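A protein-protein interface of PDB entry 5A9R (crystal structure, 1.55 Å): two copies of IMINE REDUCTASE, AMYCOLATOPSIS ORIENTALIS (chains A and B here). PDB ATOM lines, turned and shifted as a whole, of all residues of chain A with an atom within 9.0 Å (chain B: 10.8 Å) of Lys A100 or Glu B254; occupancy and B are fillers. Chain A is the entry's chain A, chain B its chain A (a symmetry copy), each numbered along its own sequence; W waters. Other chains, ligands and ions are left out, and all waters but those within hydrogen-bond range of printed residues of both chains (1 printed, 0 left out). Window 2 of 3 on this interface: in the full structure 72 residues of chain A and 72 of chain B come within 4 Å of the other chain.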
ATOM      1  N   SER A  96      13.957 -17.154   2.485  1.00  0.00           N
ATOM      2  CA  SER A  96      13.175 -18.278   2.027  1.00  0.00           C
ATOM      3  C   SER A  96      11.922 -17.701   1.359  1.00  0.00           C
ATOM      4  O   SER A  96      11.428 -16.726   1.755  1.00  0.00           O
ATOM      5  CB  SER A  96      12.777 -19.199   3.156  1.00  0.00           C
ATOM      6  OG  SER A  96      13.859 -19.926   3.562  1.00  0.00           O
ATOM      7  N   GLY A  97      11.415 -18.348   0.350  1.00  0.00           N
ATOM      8  CA  GLY A  97      10.313 -17.754  -0.371  1.00  0.00           C
ATOM      9  C   GLY A  97       8.974 -18.127   0.217  1.00  0.00           C
ATOM     10  O   GLY A  97       7.999 -17.326   0.171  1.00  0.00           O
ATOM     11  N   THR A  98       8.870 -19.350   0.715  1.00  0.00           N
ATOM     12  CA  THR A  98       7.633 -19.913   1.218  1.00  0.00           C
ATOM     13  C   THR A  98       7.950 -20.717   2.455  1.00  0.00           C
ATOM     14  O   THR A  98       9.118 -21.165   2.672  1.00  0.00           O
ATOM     15  CB  THR A  98       6.915 -20.879   0.218  1.00  0.00           C
ATOM     16  OG1 THR A  98       7.735 -22.027  -0.053  1.00  0.00           O
ATOM     17  CG2 THR A  98       6.658 -20.215  -1.091  1.00  0.00           C
ATOM     18  N   PRO A  99       6.961 -20.975   3.283  1.00  0.00           N
ATOM     19  CA  PRO A  99       7.187 -21.869   4.428  1.00  0.00           C
ATOM     20  C   PRO A  99       7.667 -23.233   4.010  1.00  0.00           C
ATOM     21  O   PRO A  99       8.563 -23.811   4.687  1.00  0.00           O
ATOM     22  CB  PRO A  99       5.774 -21.968   5.053  1.00  0.00           C
ATOM     23  CG  PRO A  99       5.180 -20.604   4.720  1.00  0.00           C
ATOM     24  CD  PRO A  99       5.575 -20.432   3.301  1.00  0.00           C
ATOM     25  N   LYS A 100       7.203 -23.768   2.880  1.00  0.00           N
ATOM     26  CA  LYS A 100       7.629 -25.105   2.469  1.00  0.00           C
ATOM     27  C   LYS A 100       9.104 -25.015   2.051  1.00  0.00           C
ATOM     28  O   LYS A 100       9.866 -25.968   2.319  1.00  0.00           O
ATOM     29  CB  LYS A 100       6.759 -25.650   1.277  1.00  0.00           C
ATOM     30  CG  LYS A 100       7.323 -26.894   0.623  1.00  0.00           C
ATOM     31  N   GLU A 101       9.558 -23.953   1.388  1.00  0.00           N
ATOM     32  CA  GLU A 101      10.980 -23.861   1.025  1.00  0.00           C
ATOM     33  C   GLU A 101      11.819 -23.817   2.306  1.00  0.00           C
ATOM     34  O   GLU A 101      12.902 -24.410   2.353  1.00  0.00           O
ATOM     35  CB  GLU A 101      11.355 -22.665   0.168  1.00  0.00           C
ATOM     36  CG  GLU A 101      10.924 -22.753  -1.277  1.00  0.00           C
ATOM     37  CD  GLU A 101      11.285 -21.468  -2.016  1.00  0.00           C
ATOM     38  OE1 GLU A 101      12.484 -21.055  -2.017  1.00  0.00           O
ATOM     39  OE2 GLU A 101      10.363 -20.839  -2.539  1.00  0.00           O
ATOM     40  N   ALA A 102      11.388 -23.084   3.353  1.00  0.00           N
ATOM     41  CA  ALA A 102      12.150 -23.063   4.592  1.00  0.00           C
ATOM     42  C   ALA A 102      12.198 -24.451   5.188  1.00  0.00           C
ATOM     43  O   ALA A 102      13.232 -24.844   5.717  1.00  0.00           O
ATOM     44  CB  ALA A 102      11.529 -22.100   5.604  1.00  0.00           C
ATOM     45  N   ASN A 103      11.067 -25.163   5.207  1.00  0.00           N
ATOM     46  CA  ASN A 103      11.082 -26.506   5.807  1.00  0.00           C
ATOM     47  C   ASN A 103      12.019 -27.440   4.993  1.00  0.00           C
ATOM     48  O   ASN A 103      12.758 -28.215   5.620  1.00  0.00           O
ATOM     49  CB  ASN A 103       9.686 -27.074   5.947  1.00  0.00           C
ATOM     50  CG  ASN A 103       8.813 -26.313   7.007  1.00  0.00           C
ATOM     51  OD1 ASN A 103       9.297 -25.783   8.047  1.00  0.00           O
ATOM     52  ND2 ASN A 103       7.540 -26.214   6.723  1.00  0.00           N
ATOM     53  N   GLU A 104      12.032 -27.349   3.688  1.00  0.00           N
ATOM     54  CA  GLU A 104      12.984 -28.160   2.797  1.00  0.00           C
ATOM     55  C   GLU A 104      14.416 -27.792   3.137  1.00  0.00           C
ATOM     56  O   GLU A 104      15.360 -28.666   3.171  1.00  0.00           O
ATOM     57  CB  GLU A 104      12.696 -27.936   1.305  1.00  0.00           C
ATOM     58  CG  GLU A 104      11.339 -28.514   0.919  1.00  0.00           C
ATOM     59  CD  GLU A 104      10.822 -28.095  -0.443  1.00  0.00           C
ATOM     60  OE1 GLU A 104      11.311 -27.127  -1.091  1.00  0.00           O
ATOM     61  OE2 GLU A 104       9.873 -28.783  -0.872  1.00  0.00           O
ATOM     62  N   ALA A 105      14.658 -26.497   3.285  1.00  0.00           N
ATOM     63  CA  ALA A 105      16.034 -26.070   3.582  1.00  0.00           C
ATOM     64  C   ALA A 105      16.532 -26.596   4.911  1.00  0.00           C
ATOM     65  O   ALA A 105      17.701 -27.000   5.015  1.00  0.00           O
ATOM     66  CB  ALA A 105      16.117 -24.574   3.595  1.00  0.00           C
ATOM     67  N   LEU A 106      15.699 -26.553   5.955  1.00  0.00           N
ATOM     68  CA  LEU A 106      16.108 -27.104   7.245  1.00  0.00           C
ATOM     69  C   LEU A 106      16.482 -28.586   7.088  1.00  0.00           C
ATOM     70  O   LEU A 106      17.499 -29.025   7.648  1.00  0.00           O
ATOM     71  CB  LEU A 106      15.031 -26.944   8.300  1.00  0.00           C
ATOM     72  CG  LEU A 106      15.415 -27.491   9.669  1.00  0.00           C
ATOM     73  CD1 LEU A 106      14.843 -26.628  10.766  1.00  0.00           C
ATOM     74  CD2 LEU A 106      14.950 -28.898   9.900  1.00  0.00           C
ATOM     75  N   ARG A 107      15.633 -29.336   6.389  1.00  0.00           N
ATOM     76  CA  ARG A 107      15.938 -30.809   6.133  1.00  0.00           C
ATOM     77  C   ARG A 107      17.232 -30.976   5.390  1.00  0.00           C
ATOM     78  O   ARG A 107      18.002 -31.912   5.728  1.00  0.00           O
ATOM     79  CB  ARG A 107      14.761 -31.483   5.382  1.00  0.00           C
ATOM     80  CG  ARG A 107      13.570 -31.759   6.327  1.00  0.00           C
ATOM     81  CD  ARG A 107      12.422 -32.559   5.677  1.00  0.00           C
ATOM     82  NE  ARG A 107      11.969 -32.037   4.382  1.00  0.00           N
ATOM     83  CZ  ARG A 107      12.429 -32.368   3.159  1.00  0.00           C
ATOM     84  NH1 ARG A 107      13.394 -33.278   2.968  1.00  0.00           N
ATOM     85  NH2 ARG A 107      11.901 -31.769   2.089  1.00  0.00           N
ATOM     86  N   TRP A 108      17.517 -30.130   4.404  1.00  0.00           N
ATOM     87  CA  TRP A 108      18.754 -30.215   3.659  1.00  0.00           C
ATOM     88  C   TRP A 108      19.941 -29.957   4.567  1.00  0.00           C
ATOM     89  O   TRP A 108      20.943 -30.716   4.624  1.00  0.00           O
ATOM     90  CB  TRP A 108      18.744 -29.244   2.492  1.00  0.00           C
ATOM     91  CG  TRP A 108      19.847 -29.385   1.577  1.00  0.00           C
ATOM     92  CD1 TRP A 108      19.944 -30.312   0.542  1.00  0.00           C
ATOM     93  CD2 TRP A 108      21.047 -28.623   1.520  1.00  0.00           C
ATOM     94  NE1 TRP A 108      21.116 -30.161  -0.117  1.00  0.00           N
ATOM     95  CE2 TRP A 108      21.811 -29.119   0.455  1.00  0.00           C
ATOM     96  CE3 TRP A 108      21.529 -27.573   2.237  1.00  0.00           C
ATOM     97  CZ2 TRP A 108      23.083 -28.598   0.129  1.00  0.00           C
ATOM     98  CZ3 TRP A 108      22.809 -27.011   1.875  1.00  0.00           C
ATOM     99  CH2 TRP A 108      23.563 -27.562   0.894  1.00  0.00           C
ATOM    100  N   TYR A 116      20.343 -24.949  11.550  1.00  0.00           N
ATOM    101  CA  TYR A 116      19.529 -24.104  10.693  1.00  0.00           C
ATOM    102  C   TYR A 116      18.538 -23.223  11.423  1.00  0.00           C
ATOM    103  O   TYR A 116      17.760 -23.707  12.234  1.00  0.00           O
ATOM    104  CB  TYR A 116      18.807 -24.923   9.671  1.00  0.00           C
ATOM    105  CG  TYR A 116      18.070 -24.168   8.588  1.00  0.00           C
ATOM    106  CD1 TYR A 116      16.767 -23.786   8.782  1.00  0.00           C
ATOM    107  CD2 TYR A 116      18.671 -23.849   7.375  1.00  0.00           C
ATOM    108  CE1 TYR A 116      16.107 -23.041   7.790  1.00  0.00           C
ATOM    109  CE2 TYR A 116      18.045 -23.104   6.409  1.00  0.00           C
ATOM    110  CZ  TYR A 116      16.746 -22.728   6.595  1.00  0.00           C
ATOM    111  OH  TYR A 116      16.093 -21.961   5.628  1.00  0.00           O
ATOM    112  N   ASP A 118      15.694 -20.021  10.181  1.00  0.00           N
ATOM    113  CA  ASP A 118      15.123 -19.256   9.097  1.00  0.00           C
ATOM    114  C   ASP A 118      14.714 -17.927   9.698  1.00  0.00           C
ATOM    115  O   ASP A 118      14.380 -17.883  10.869  1.00  0.00           O
ATOM    116  CB  ASP A 118      13.903 -19.937   8.515  1.00  0.00           C
ATOM    117  CG  ASP A 118      13.686 -19.585   7.081  1.00  0.00           C
ATOM    118  OD1 ASP A 118      14.383 -20.106   6.181  1.00  0.00           O
ATOM    119  OD2 ASP A 118      12.854 -18.676   6.754  1.00  0.00           O
ATOM    120  N   ALA A 164      10.469 -24.590  10.833  1.00  0.00           N
ATOM    121  CA  ALA A 164      11.308 -23.648  10.081  1.00  0.00           C
ATOM    122  C   ALA A 164      10.485 -22.655   9.302  1.00  0.00           C
ATOM    123  O   ALA A 164      10.943 -21.518   9.156  1.00  0.00           O
ATOM    124  CB  ALA A 164      12.324 -24.319   9.163  1.00  0.00           C
ATOM    125  N   GLY A 165       9.289 -23.041   8.846  1.00  0.00           N
ATOM    126  CA  GLY A 165       8.471 -22.123   7.990  1.00  0.00           C
ATOM    127  C   GLY A 165       7.708 -21.068   8.754  1.00  0.00           C
ATOM    128  O   GLY A 165       7.035 -20.239   8.087  1.00  0.00           O
ATOM    129  N   LEU A 166       7.799 -20.976  10.081  1.00  0.00           N
ATOM    130  CA  LEU A 166       6.968 -20.052  10.819  1.00  0.00           C
ATOM    131  C   LEU A 166       7.304 -18.596  10.567  1.00  0.00           C
ATOM    132  O   LEU A 166       6.412 -17.684  10.494  1.00  0.00           O
ATOM    133  CB  LEU A 166       7.072 -20.299  12.328  1.00  0.00           C
ATOM    134  CG  LEU A 166       6.002 -20.469  13.362  1.00  0.00           C
ATOM    135  CD1 LEU A 166       4.718 -21.117  12.813  1.00  0.00           C
ATOM    136  CD2 LEU A 166       6.633 -21.328  14.480  1.00  0.00           C
ATOM    137  N   VAL A 168       8.560 -17.147   7.784  1.00  0.00           N
ATOM    138  CA  VAL A 168       8.026 -16.743   6.484  1.00  0.00           C
ATOM    139  C   VAL A 168       6.480 -16.618   6.589  1.00  0.00           C
ATOM    140  O   VAL A 168       5.919 -15.641   6.095  1.00  0.00           O
ATOM    141  CB  VAL A 168       8.371 -17.747   5.385  1.00  0.00           C
ATOM    142  CG1 VAL A 168       7.545 -17.495   4.125  1.00  0.00           C
ATOM    143  CG2 VAL A 168       9.814 -17.621   5.053  1.00  0.00           C
ATOM    144  N   LEU A 169       5.857 -17.501   7.338  1.00  0.00           N
ATOM    145  CA  LEU A 169       4.412 -17.443   7.485  1.00  0.00           C
ATOM    146  C   LEU A 169       3.986 -16.164   8.222  1.00  0.00           C
ATOM    147  O   LEU A 169       3.031 -15.457   7.801  1.00  0.00           O
ATOM    148  CB  LEU A 169       3.872 -18.730   8.111  1.00  0.00           C
ATOM    149  CG  LEU A 169       2.375 -18.858   8.257  1.00  0.00           C
ATOM    150  CD1 LEU A 169       1.765 -18.902   6.848  1.00  0.00           C
ATOM    151  CD2 LEU A 169       2.051 -20.065   9.101  1.00  0.00           C
ATOM    152  N   HIS B 187      -7.243 -11.979   7.668  1.00  0.00           N
ATOM    153  CA  HIS B 187      -6.491 -12.805   6.722  1.00  0.00           C
ATOM    154  C   HIS B 187      -5.157 -13.273   7.315  1.00  0.00           C
ATOM    155  O   HIS B 187      -4.775 -14.435   7.210  1.00  0.00           O
ATOM    156  CB  HIS B 187      -6.278 -12.039   5.396  1.00  0.00           C
ATOM    157  CG  HIS B 187      -5.661 -12.873   4.376  1.00  0.00           C
ATOM    158  ND1 HIS B 187      -4.364 -12.749   3.982  1.00  0.00           N
ATOM    159  CD2 HIS B 187      -6.158 -13.968   3.729  1.00  0.00           C
ATOM    160  CE1 HIS B 187      -4.081 -13.715   3.127  1.00  0.00           C
ATOM    161  NE2 HIS B 187      -5.129 -14.488   2.996  1.00  0.00           N
ATOM    162  N   ALA B 190      -5.918 -16.010   9.803  1.00  0.00           N
ATOM    163  CA  ALA B 190      -6.150 -17.244   9.079  1.00  0.00           C
ATOM    164  C   ALA B 190      -4.836 -17.913   8.628  1.00  0.00           C
ATOM    165  O   ALA B 190      -4.690 -19.156   8.701  1.00  0.00           O
ATOM    166  CB  ALA B 190      -7.097 -17.040   7.922  1.00  0.00           C
ATOM    167  N   LEU B 191      -3.938 -17.074   8.121  1.00  0.00           N
ATOM    168  CA  LEU B 191      -2.630 -17.558   7.678  1.00  0.00           C
ATOM    169  C   LEU B 191      -1.803 -18.189   8.796  1.00  0.00           C
ATOM    170  O   LEU B 191      -1.418 -19.377   8.710  1.00  0.00           O
ATOM    171  CB  LEU B 191      -1.781 -16.475   7.043  1.00  0.00           C
ATOM    172  CG  LEU B 191      -2.119 -16.132   5.630  1.00  0.00           C
ATOM    173  CD1 LEU B 191      -1.554 -14.801   5.174  1.00  0.00           C
ATOM    174  CD2 LEU B 191      -1.665 -17.279   4.703  1.00  0.00           C
ATOM    175  N   SER B 194      -3.385 -21.519  10.115  1.00  0.00           N
ATOM    176  CA  SER B 194      -3.181 -22.714   9.328  1.00  0.00           C
ATOM    177  C   SER B 194      -1.965 -23.468   9.817  1.00  0.00           C
ATOM    178  O   SER B 194      -1.849 -24.638   9.477  1.00  0.00           O
ATOM    179  CB  SER B 194      -3.072 -22.349   7.836  1.00  0.00           C
ATOM    180  OG  SER B 194      -1.819 -21.765   7.538  1.00  0.00           O
ATOM    181  N   ALA B 195      -1.107 -22.908  10.687  1.00  0.00           N
ATOM    182  CA  ALA B 195      -0.014 -23.589  11.312  1.00  0.00           C
ATOM    183  C   ALA B 195      -0.236 -23.800  12.807  1.00  0.00           C
ATOM    184  O   ALA B 195       0.694 -24.152  13.542  1.00  0.00           O
ATOM    185  CB  ALA B 195       1.255 -22.869  11.049  1.00  0.00           C
ATOM    186  N   LYS B 246       2.024 -10.833  -4.999  1.00  0.00           N
ATOM    187  CA  LYS B 246       2.058 -12.195  -5.610  1.00  0.00           C
ATOM    188  C   LYS B 246       2.629 -13.285  -4.719  1.00  0.00           C
ATOM    189  O   LYS B 246       2.081 -14.445  -4.699  1.00  0.00           O
ATOM    190  CB  LYS B 246       2.894 -12.149  -6.900  1.00  0.00           C
ATOM    191  CG  LYS B 246       2.171 -11.437  -7.994  1.00  0.00           C
ATOM    192  CD  LYS B 246       3.137 -11.242  -9.188  1.00  0.00           C
ATOM    193  CE  LYS B 246       2.355 -10.597 -10.240  1.00  0.00           C
ATOM    194  NZ  LYS B 246       3.166 -10.275 -11.445  1.00  0.00           N
ATOM    195  N   HIS B 247       3.698 -12.994  -3.980  1.00  0.00           N
ATOM    196  CA  HIS B 247       4.282 -13.944  -3.026  1.00  0.00           C
ATOM    197  C   HIS B 247       3.276 -14.261  -1.895  1.00  0.00           C
ATOM    198  O   HIS B 247       3.138 -15.391  -1.466  1.00  0.00           O
ATOM    199  CB  HIS B 247       5.554 -13.472  -2.451  1.00  0.00           C
ATOM    200  CG  HIS B 247       6.647 -13.300  -3.475  1.00  0.00           C
ATOM    201  ND1 HIS B 247       7.838 -12.649  -3.230  1.00  0.00           N
ATOM    202  CD2 HIS B 247       6.701 -13.681  -4.775  1.00  0.00           C
ATOM    203  CE1 HIS B 247       8.586 -12.644  -4.317  1.00  0.00           C
ATOM    204  NE2 HIS B 247       7.913 -13.242  -5.277  1.00  0.00           N
ATOM    205  N   ILE B 248       2.637 -13.221  -1.351  1.00  0.00           N
ATOM    206  CA  ILE B 248       1.580 -13.440  -0.325  1.00  0.00           C
ATOM    207  C   ILE B 248       0.505 -14.376  -0.835  1.00  0.00           C
ATOM    208  O   ILE B 248       0.074 -15.316  -0.079  1.00  0.00           O
ATOM    209  CB  ILE B 248       0.979 -12.097   0.145  1.00  0.00           C
ATOM    210  CG1 ILE B 248       2.066 -11.310   0.918  1.00  0.00           C
ATOM    211  CG2 ILE B 248      -0.280 -12.322   1.021  1.00  0.00           C
ATOM    212  CD1 ILE B 248       1.675  -9.858   1.140  1.00  0.00           C
ATOM    213  N   ILE B 249       0.020 -14.113  -2.040  1.00  0.00           N
ATOM    214  CA  ILE B 249      -1.006 -14.991  -2.680  1.00  0.00           C
ATOM    215  C   ILE B 249      -0.463 -16.411  -2.753  1.00  0.00           C
ATOM    216  O   ILE B 249      -1.178 -17.343  -2.415  1.00  0.00           O
ATOM    217  CB  ILE B 249      -1.458 -14.444  -4.066  1.00  0.00           C
ATOM    218  CG1 ILE B 249      -2.147 -13.114  -3.892  1.00  0.00           C
ATOM    219  CG2 ILE B 249      -2.401 -15.450  -4.677  1.00  0.00           C
ATOM    220  CD1 ILE B 249      -2.220 -12.281  -5.175  1.00  0.00           C
ATOM    221  N   GLY B 250       0.748 -16.613  -3.277  1.00  0.00           N
ATOM    222  CA  GLY B 250       1.251 -17.994  -3.361  1.00  0.00           C
ATOM    223  C   GLY B 250       1.419 -18.711  -2.056  1.00  0.00           C
ATOM    224  O   GLY B 250       1.081 -19.884  -1.960  1.00  0.00           O
ATOM    225  N   THR B 251       1.958 -18.024  -1.027  1.00  0.00           N
ATOM    226  CA  THR B 251       2.017 -18.567   0.312  1.00  0.00           C
ATOM    227  C   THR B 251       0.632 -18.917   0.844  1.00  0.00           C
ATOM    228  O   THR B 251       0.472 -20.012   1.455  1.00  0.00           O
ATOM    229  CB  THR B 251       2.857 -17.678   1.253  1.00  0.00           C
ATOM    230  OG1 THR B 251       4.215 -17.773   0.816  1.00  0.00           O
ATOM    231  CG2 THR B 251       2.808 -18.101   2.665  1.00  0.00           C
ATOM    232  N   SER B 252      -0.348 -18.007   0.669  1.00  0.00           N
ATOM    233  CA  SER B 252      -1.704 -18.299   1.128  1.00  0.00           C
ATOM    234  C   SER B 252      -2.246 -19.601   0.444  1.00  0.00           C
ATOM    235  O   SER B 252      -2.859 -20.472   1.078  1.00  0.00           O
ATOM    236  CB  SER B 252      -2.602 -17.079   0.889  1.00  0.00           C
ATOM    237  OG  SER B 252      -3.805 -17.107   1.662  1.00  0.00           O
ATOM    238  N   GLN B 253      -1.994 -19.752  -0.853  1.00  0.00           N
ATOM    239  CA  GLN B 253      -2.451 -20.911  -1.561  1.00  0.00           C
ATOM    240  C   GLN B 253      -1.811 -22.185  -1.052  1.00  0.00           C
ATOM    241  O   GLN B 253      -2.498 -23.171  -0.765  1.00  0.00           O
ATOM    242  CB  GLN B 253      -2.146 -20.776  -3.066  1.00  0.00           C
ATOM    243  CG  GLN B 253      -2.977 -19.730  -3.792  1.00  0.00           C
ATOM    244  CD  GLN B 253      -2.688 -19.713  -5.311  1.00  0.00           C
ATOM    245  OE1 GLN B 253      -1.986 -20.604  -5.829  1.00  0.00           O
ATOM    246  NE2 GLN B 253      -3.293 -18.811  -6.012  1.00  0.00           N
ATOM    247  N   GLU B 254      -0.514 -22.129  -0.764  1.00  0.00           N
ATOM    248  CA  GLU B 254       0.192 -23.298  -0.222  1.00  0.00           C
ATOM    249  C   GLU B 254      -0.307 -23.702   1.151  1.00  0.00           C
ATOM    250  O   GLU B 254      -0.230 -24.863   1.543  1.00  0.00           O
ATOM    251  CB  GLU B 254       1.708 -23.134  -0.205  1.00  0.00           C
ATOM    252  CG  GLU B 254       2.313 -23.025  -1.591  1.00  0.00           C
ATOM    253  CD  GLU B 254       3.803 -23.313  -1.650  1.00  0.00           C
ATOM    254  OE1 GLU B 254       4.466 -23.459  -0.603  1.00  0.00           O
ATOM    255  OE2 GLU B 254       4.289 -23.383  -2.785  1.00  0.00           O
ATOM    256  N   GLN B 255      -0.740 -22.726   1.949  1.00  0.00           N
ATOM    257  CA  GLN B 255      -1.297 -22.996   3.290  1.00  0.00           C
ATOM    258  C   GLN B 255      -2.750 -23.361   3.258  1.00  0.00           C
ATOM    259  O   GLN B 255      -3.347 -23.648   4.291  1.00  0.00           O
ATOM    260  CB  GLN B 255      -1.125 -21.730   4.212  1.00  0.00           C
ATOM    261  CG  GLN B 255       0.330 -21.381   4.480  1.00  0.00           C
ATOM    262  CD  GLN B 255       1.060 -22.435   5.220  1.00  0.00           C
ATOM    263  OE1 GLN B 255       2.048 -22.927   4.720  1.00  0.00           O
ATOM    264  NE2 GLN B 255       0.497 -22.890   6.378  1.00  0.00           N
ATOM    265  N   GLY B 256      -3.366 -23.358   2.090  1.00  0.00           N
ATOM    266  CA  GLY B 256      -4.805 -23.603   2.024  1.00  0.00           C
ATOM    267  C   GLY B 256      -5.724 -22.554   2.550  1.00  0.00           C
ATOM    268  O   GLY B 256      -6.855 -22.896   3.012  1.00  0.00           O
ATOM    269  N   VAL B 257      -5.288 -21.294   2.524  1.00  0.00           N
ATOM    270  CA  VAL B 257      -5.991 -20.147   3.018  1.00  0.00           C
ATOM    271  C   VAL B 257      -6.522 -19.319   1.858  1.00  0.00           C
ATOM    272  O   VAL B 257      -5.796 -19.123   0.870  1.00  0.00           O
ATOM    273  CB  VAL B 257      -5.066 -19.305   3.992  1.00  0.00           C
ATOM    274  CG1 VAL B 257      -5.744 -18.021   4.381  1.00  0.00           C
ATOM    275  CG2 VAL B 257      -4.815 -20.168   5.191  1.00  0.00           C
ATOM    276  N   ASP B 258      -7.755 -18.854   1.957  1.00  0.00           N
ATOM    277  CA  ASP B 258      -8.450 -18.137   0.886  1.00  0.00           C
ATOM    278  C   ASP B 258      -7.663 -16.920   0.483  1.00  0.00           C
ATOM    279  O   ASP B 258      -6.999 -16.322   1.324  1.00  0.00           O
ATOM    280  CB  ASP B 258      -9.796 -17.674   1.363  1.00  0.00           C
ATOM    281  CG  ASP B 258     -10.579 -16.938   0.306  1.00  0.00           C
ATOM    282  OD1 ASP B 258     -11.261 -17.681  -0.354  1.00  0.00           O
ATOM    283  OD2 ASP B 258     -10.586 -15.686   0.206  1.00  0.00           O
ATOM    284  N   THR B 259      -7.602 -16.614  -0.789  1.00  0.00           N
ATOM    285  CA  THR B 259      -6.697 -15.560  -1.281  1.00  0.00           C
ATOM    286  C   THR B 259      -7.422 -14.283  -1.604  1.00  0.00           C
ATOM    287  O   THR B 259      -6.797 -13.359  -2.116  1.00  0.00           O
ATOM    288  CB  THR B 259      -5.984 -16.017  -2.618  1.00  0.00           C
ATOM    289  OG1 THR B 259      -7.015 -16.365  -3.570  1.00  0.00           O
ATOM    290  CG2 THR B 259      -5.110 -17.215  -2.364  1.00  0.00           C
ATOM    291  N   PRO B 262      -5.616 -10.700  -0.348  1.00  0.00           N
ATOM    292  CA  PRO B 262      -4.468 -10.285  -1.128  1.00  0.00           C
ATOM    293  C   PRO B 262      -4.753 -10.108  -2.608  1.00  0.00           C
ATOM    294  O   PRO B 262      -4.121  -9.256  -3.231  1.00  0.00           O
ATOM    295  CB  PRO B 262      -3.377 -11.320  -0.798  1.00  0.00           C
ATOM    296  CG  PRO B 262      -4.194 -12.514  -0.349  1.00  0.00           C
ATOM    297  CD  PRO B 262      -5.390 -11.984   0.361  1.00  0.00           C
HETATM  298  O   HOH W   1       6.986 -23.337  -2.027  1.00  0.00           O
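Water W1 bridges the side-chain hydroxyl (OG1) of Thr A98 and the side-chain carboxylate (OE2) of Glu B254.
Of chain B, only Glu B254 comes within 4 Å of Lys A100.
No residue of chain B comes within 4 Å of Ala A102.
No residue of chain B comes within 4 Å of Asn A103.
No residue of chain B comes within 4 Å of Glu A104.
Ala A164 touches none of the printed residues of chain B.
No residue of chain B comes within 4 Å of Gly A165.
Printed residues of chain B within 4 Å of Leu A169: Leu B191 (3.6 Å), Ala B195 (3.5 Å) and Gln B255 (3.7 Å).
Of the printed residues of chain A, Leu B191 touches Leu A169 (3.6 Å).
Printed residues of chain A within 4 Å of Thr B251: Gly A97, Thr A98 and Pro A99.
Printed residues of chain A within 4 Å of Glu B254: Thr A98 and Lys A100.
Of the printed residues of chain A, Gln B255 touches Pro A99 (3.9 Å) and Leu A169 (3.7 Å).
Gly B256 touches none of the printed residues of chain A.
The nearest printed residue of chain A that does not touch Gln B255 is Lys A100 (5.5 Å).
The side-chain hydroxyl (OG1) of Thr A98 sits close to the backbone NH (N) of Lys A100, at 3.5 Å.
The side-chain hydroxyl (OG1) of Thr A98 sits at hydrogen-bond distance from the backbone NH (N) of Glu A101 (3.0 Å).
The backbone carbonyl oxygen (O) of Pro A99 lies within hydrogen-bond range of the side-chain amide nitrogen (ND2) of Asn A103 (3.3 Å).
The backbone carbonyl oxygen of Leu B191 is in hydrogen-bond range of the side-chain hydroxyl of Ser B194, at 2.7 Å.
The side-chain hydroxyl (OG) of Ser B194 lies within hydrogen-bond range of the side-chain amide nitrogen (NE2) of Gln B255 (2.8 Å).
The backbone carbonyl oxygen (O) of His B247 is in hydrogen-bond range of the side-chain hydroxyl (OG1) of Thr B251 (3.5 Å).
Among the printed residues, merely in contact across the chains: Leu A169 with Ala B195 (3.5 Å), Leu A169 with Leu B191 (3.6 Å), Thr A98 with Glu B254 (3.6 Å), Pro A99 with Thr B251 (3.7 Å), Lys A100 with Glu B254 (3.7 Å), Leu A169 with Gln B255 (3.7 Å), Pro A99 with Gln B255 (3.9 Å), Gly A97 with Thr B251 (3.9 Å) and Thr A98 with Thr B251 (3.9 Å).
Hydrophobic or aromatic side chains of chain B that line the printed part of chain A: Ala B195.
Among the printed residues, 9 pairs touch across the chains.
Among the printed residues, no Asp or Glu carboxylate lies within 4 Å of a Lys or Arg side-chain nitrogen of the other chain.
No position is printed for both chains.
Of the 9 pairs that touch across the chains among the printed residues, none has its exchanged pair printed and touching as well.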
